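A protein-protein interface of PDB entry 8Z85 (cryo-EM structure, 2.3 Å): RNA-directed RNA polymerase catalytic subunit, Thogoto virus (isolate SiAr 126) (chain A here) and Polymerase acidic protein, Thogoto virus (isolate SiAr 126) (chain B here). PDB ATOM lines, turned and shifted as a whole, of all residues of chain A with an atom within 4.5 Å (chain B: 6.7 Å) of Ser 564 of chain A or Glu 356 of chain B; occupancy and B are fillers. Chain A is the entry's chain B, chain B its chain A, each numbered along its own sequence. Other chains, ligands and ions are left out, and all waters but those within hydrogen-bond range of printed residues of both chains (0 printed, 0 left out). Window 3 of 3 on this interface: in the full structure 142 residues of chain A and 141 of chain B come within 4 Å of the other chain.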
ATOM      1  N   ARG A 527      24.710 -13.770   3.038  1.00  0.00           N
ATOM      2  CA  ARG A 527      24.651 -12.653   2.102  1.00  0.00           C
ATOM      3  C   ARG A 527      23.308 -11.944   2.178  1.00  0.00           C
ATOM      4  O   ARG A 527      23.249 -10.710   2.188  1.00  0.00           O
ATOM      5  CB  ARG A 527      24.909 -13.146   0.680  1.00  0.00           C
ATOM      6  CG  ARG A 527      26.370 -13.249   0.284  1.00  0.00           C
ATOM      7  CD  ARG A 527      26.469 -13.606  -1.187  1.00  0.00           C
ATOM      8  NE  ARG A 527      27.783 -13.338  -1.760  1.00  0.00           N
ATOM      9  CZ  ARG A 527      28.787 -14.202  -1.761  1.00  0.00           C
ATOM     10  NH1 ARG A 527      28.685 -15.384  -1.179  1.00  0.00           N
ATOM     11  NH2 ARG A 527      29.926 -13.870  -2.363  1.00  0.00           N
ATOM     12  N   ASN A 530      23.279 -10.569   5.965  1.00  0.00           N
ATOM     13  CA  ASN A 530      24.221  -9.473   6.174  1.00  0.00           C
ATOM     14  C   ASN A 530      23.773  -8.212   5.450  1.00  0.00           C
ATOM     15  O   ASN A 530      23.871  -7.106   5.992  1.00  0.00           O
ATOM     16  CB  ASN A 530      25.619  -9.886   5.713  1.00  0.00           C
ATOM     17  CG  ASN A 530      26.572  -8.714   5.616  1.00  0.00           C
ATOM     18  OD1 ASN A 530      27.177  -8.312   6.608  1.00  0.00           O
ATOM     19  ND2 ASN A 530      26.717  -8.163   4.417  1.00  0.00           N
ATOM     20  N   LYS A 534      22.703  -4.935   7.451  1.00  0.00           N
ATOM     21  CA  LYS A 534      23.289  -3.616   7.237  1.00  0.00           C
ATOM     22  C   LYS A 534      22.222  -2.570   6.942  1.00  0.00           C
ATOM     23  O   LYS A 534      22.324  -1.428   7.405  1.00  0.00           O
ATOM     24  CB  LYS A 534      24.305  -3.673   6.098  1.00  0.00           C
ATOM     25  CG  LYS A 534      25.619  -4.329   6.471  1.00  0.00           C
ATOM     26  CD  LYS A 534      26.648  -4.144   5.372  1.00  0.00           C
ATOM     27  CE  LYS A 534      27.980  -4.754   5.762  1.00  0.00           C
ATOM     28  NZ  LYS A 534      29.077  -4.290   4.870  1.00  0.00           N
ATOM     29  N   GLY A 562      29.056  -0.746   8.056  1.00  0.00           N
ATOM     30  CA  GLY A 562      29.250  -0.804   6.625  1.00  0.00           C
ATOM     31  C   GLY A 562      30.548  -1.439   6.179  1.00  0.00           C
ATOM     32  O   GLY A 562      30.816  -1.471   4.972  1.00  0.00           O
ATOM     33  N   ALA A 563      31.357  -1.943   7.105  1.00  0.00           N
ATOM     34  CA  ALA A 563      32.593  -2.614   6.737  1.00  0.00           C
ATOM     35  C   ALA A 563      32.291  -3.968   6.098  1.00  0.00           C
ATOM     36  O   ALA A 563      31.179  -4.494   6.178  1.00  0.00           O
ATOM     37  CB  ALA A 563      33.493  -2.788   7.958  1.00  0.00           C
ATOM     38  N   SER A 564      33.305  -4.529   5.448  1.00  0.00           N
ATOM     39  CA  SER A 564      33.140  -5.818   4.795  1.00  0.00           C
ATOM     40  C   SER A 564      32.818  -6.888   5.836  1.00  0.00           C
ATOM     41  O   SER A 564      33.351  -6.849   6.951  1.00  0.00           O
ATOM     42  CB  SER A 564      34.405  -6.196   4.025  1.00  0.00           C
ATOM     43  OG  SER A 564      34.816  -5.145   3.170  1.00  0.00           O
ATOM     44  N   PRO A 565      31.950  -7.849   5.514  1.00  0.00           N
ATOM     45  CA  PRO A 565      31.597  -8.888   6.492  1.00  0.00           C
ATOM     46  C   PRO A 565      32.810  -9.744   6.825  1.00  0.00           C
ATOM     47  O   PRO A 565      33.461 -10.297   5.936  1.00  0.00           O
ATOM     48  CB  PRO A 565      30.506  -9.693   5.778  1.00  0.00           C
ATOM     49  CG  PRO A 565      30.765  -9.470   4.331  1.00  0.00           C
ATOM     50  CD  PRO A 565      31.298  -8.069   4.212  1.00  0.00           C
ATOM     51  N   VAL A 566      33.114  -9.845   8.118  1.00  0.00           N
ATOM     52  CA  VAL A 566      34.307 -10.556   8.556  1.00  0.00           C
ATOM     53  C   VAL A 566      34.028 -12.029   8.835  1.00  0.00           C
ATOM     54  O   VAL A 566      34.971 -12.831   8.890  1.00  0.00           O
ATOM     55  CB  VAL A 566      34.899  -9.864   9.799  1.00  0.00           C
ATOM     56  CG1 VAL A 566      34.004 -10.073  11.015  1.00  0.00           C
ATOM     57  CG2 VAL A 566      36.329 -10.311  10.053  1.00  0.00           C
ATOM     58  N   ARG A 580      37.799  -9.940  14.654  1.00  0.00           N
ATOM     59  CA  ARG A 580      38.440  -8.828  13.958  1.00  0.00           C
ATOM     60  C   ARG A 580      39.772  -8.461  14.596  1.00  0.00           C
ATOM     61  O   ARG A 580      40.695  -8.025  13.899  1.00  0.00           O
ATOM     62  CB  ARG A 580      37.513  -7.613  13.930  1.00  0.00           C
ATOM     63  CG  ARG A 580      36.337  -7.749  12.978  1.00  0.00           C
ATOM     64  CD  ARG A 580      35.605  -6.429  12.808  1.00  0.00           C
ATOM     65  NE  ARG A 580      34.530  -6.526  11.827  1.00  0.00           N
ATOM     66  CZ  ARG A 580      34.692  -6.373  10.520  1.00  0.00           C
ATOM     67  NH1 ARG A 580      35.878  -6.106   9.996  1.00  0.00           N
ATOM     68  NH2 ARG A 580      33.639  -6.490   9.717  1.00  0.00           N
ATOM     69  N   GLU B 354      23.560  -7.725  -5.992  1.00  0.00           N
ATOM     70  CA  GLU B 354      24.861  -7.279  -5.503  1.00  0.00           C
ATOM     71  C   GLU B 354      24.890  -7.488  -3.994  1.00  0.00           C
ATOM     72  O   GLU B 354      24.578  -6.581  -3.219  1.00  0.00           O
ATOM     73  CB  GLU B 354      25.118  -5.825  -5.888  1.00  0.00           C
ATOM     74  CG  GLU B 354      25.222  -5.609  -7.391  1.00  0.00           C
ATOM     75  CD  GLU B 354      25.031  -4.161  -7.794  1.00  0.00           C
ATOM     76  OE1 GLU B 354      24.750  -3.327  -6.908  1.00  0.00           O
ATOM     77  OE2 GLU B 354      25.159  -3.857  -8.998  1.00  0.00           O
ATOM     78  N   LEU B 355      25.268  -8.694  -3.583  1.00  0.00           N
ATOM     79  CA  LEU B 355      25.400  -9.055  -2.180  1.00  0.00           C
ATOM     80  C   LEU B 355      26.879  -9.105  -1.827  1.00  0.00           C
ATOM     81  O   LEU B 355      27.676  -9.689  -2.568  1.00  0.00           O
ATOM     82  CB  LEU B 355      24.733 -10.402  -1.895  1.00  0.00           C
ATOM     83  CG  LEU B 355      23.219 -10.461  -2.106  1.00  0.00           C
ATOM     84  CD1 LEU B 355      22.724 -11.897  -2.066  1.00  0.00           C
ATOM     85  CD2 LEU B 355      22.495  -9.613  -1.074  1.00  0.00           C
ATOM     86  N   GLU B 356      27.239  -8.484  -0.706  1.00  0.00           N
ATOM     87  CA  GLU B 356      28.640  -8.398  -0.313  1.00  0.00           C
ATOM     88  C   GLU B 356      29.225  -9.785  -0.083  1.00  0.00           C
ATOM     89  O   GLU B 356      28.608 -10.634   0.566  1.00  0.00           O
ATOM     90  CB  GLU B 356      28.780  -7.545   0.947  1.00  0.00           C
ATOM     91  CG  GLU B 356      30.056  -6.723   0.996  1.00  0.00           C
ATOM     92  CD  GLU B 356      29.968  -5.574   1.979  1.00  0.00           C
ATOM     93  OE1 GLU B 356      28.947  -5.475   2.689  1.00  0.00           O
ATOM     94  OE2 GLU B 356      30.922  -4.769   2.041  1.00  0.00           O
ATOM     95  N   LYS B 357      30.421 -10.009  -0.620  1.00  0.00           N
ATOM     96  CA  LYS B 357      31.084 -11.297  -0.476  1.00  0.00           C
ATOM     97  C   LYS B 357      31.511 -11.525   0.967  1.00  0.00           C
ATOM     98  O   LYS B 357      32.047 -10.629   1.624  1.00  0.00           O
ATOM     99  CB  LYS B 357      32.300 -11.366  -1.400  1.00  0.00           C
ATOM    100  CG  LYS B 357      32.884 -12.758  -1.565  1.00  0.00           C
ATOM    101  CD  LYS B 357      33.867 -12.806  -2.723  1.00  0.00           C
ATOM    102  CE  LYS B 357      33.262 -12.219  -3.989  1.00  0.00           C
ATOM    103  NZ  LYS B 357      34.203 -12.289  -5.140  1.00  0.00           N
ATOM    104  N   ASN B 358      31.276 -12.737   1.459  1.00  0.00           N
ATOM    105  CA  ASN B 358      31.686 -13.095   2.806  1.00  0.00           C
ATOM    106  C   ASN B 358      33.189 -13.365   2.851  1.00  0.00           C
ATOM    107  O   ASN B 358      33.856 -13.511   1.824  1.00  0.00           O
ATOM    108  CB  ASN B 358      30.916 -14.318   3.299  1.00  0.00           C
ATOM    109  CG  ASN B 358      29.432 -14.051   3.453  1.00  0.00           C
ATOM    110  OD1 ASN B 358      28.613 -14.960   3.328  1.00  0.00           O
ATOM    111  ND2 ASN B 358      29.081 -12.801   3.729  1.00  0.00           N
ATOM    112  N   GLU B 369      31.821 -19.850  -1.076  1.00  0.00           N
ATOM    113  CA  GLU B 369      31.712 -18.541  -1.707  1.00  0.00           C
ATOM    114  C   GLU B 369      31.783 -18.646  -3.224  1.00  0.00           C
ATOM    115  O   GLU B 369      31.156 -17.848  -3.928  1.00  0.00           O
ATOM    116  CB  GLU B 369      32.804 -17.614  -1.180  1.00  0.00           C
ATOM    117  CG  GLU B 369      32.636 -17.267   0.287  1.00  0.00           C
ATOM    118  CD  GLU B 369      31.321 -16.569   0.567  1.00  0.00           C
ATOM    119  OE1 GLU B 369      30.939 -15.682  -0.221  1.00  0.00           O
ATOM    120  OE2 GLU B 369      30.663 -16.922   1.567  1.00  0.00           O
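OE1 of Glu 369 of chain B lies within salt-bridge range of NH1 of Arg 527 of chain A. NZ of Lys 534 of chain A is in salt-bridge range of OE1 of Glu 356 of chain B, at 2.5 Å.
NZ of Lys 534 of chain A sits at hydrogen-bond distance from O of Ala 563 of chain A, at 2.5 Å. OD1 of Asn 358 of chain B lies close to OE2 of Glu 369 of chain B. O of Ser 564 of chain A sits at hydrogen-bond distance from NH2 of Arg 580 of chain A, at 2.8 Å. The side-chain amino group of Lys 534 of chain A lies within hydrogen-bond range of the backbone carbonyl oxygen of Gly 562 of chain A, at 3.3 Å.
Among the printed residues, merely in contact across the chains: Arg 527 of chain A with Leu 355 of chain B, Arg 527 of chain A with Glu 356 of chain B, Arg 527 of chain A with Lys 357 of chain B, Asn 530 of chain A with Glu 356 of chain B, Ser 564 of chain A with Glu 356 of chain B, Pro 565 of chain A with Glu 356 of chain B, Pro 565 of chain A with Lys 357 of chain B and Pro 565 of chain A with Asn 358 of chain B.
Printed residues of chain B within 4 Å of Arg 527 of chain A: Leu 355, Glu 356, Lys 357 and Glu 369. Printed residues of chain B within 4 Å of Asn 530 of chain A: Glu 356 (3.9 Å). Printed residues of chain B within 4 Å of Lys 534 of chain A: Glu 356. Ser 564 of chain A touches one residue of chain B. Arg 580 of chain A touches none of the printed residues of chain B. Glu 354 of chain B touches none of the printed residues of chain A. Glu 356 of chain B touches five residues of chain A. Printed residues of chain A within 4 Å of Asn 358 of chain B: Pro 565. The nearest residue of chain A that does not touch Glu 356 of chain B is Ala 563 of chain A (4.2 Å).
Among the printed residues, Asp or Glu carboxylates within 4 Å of a Lys or Arg side-chain nitrogen of the other chain: Arg 527 of chain A with Glu 369 of chain B and Lys 534 of chain A with Glu 356 of chain B.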
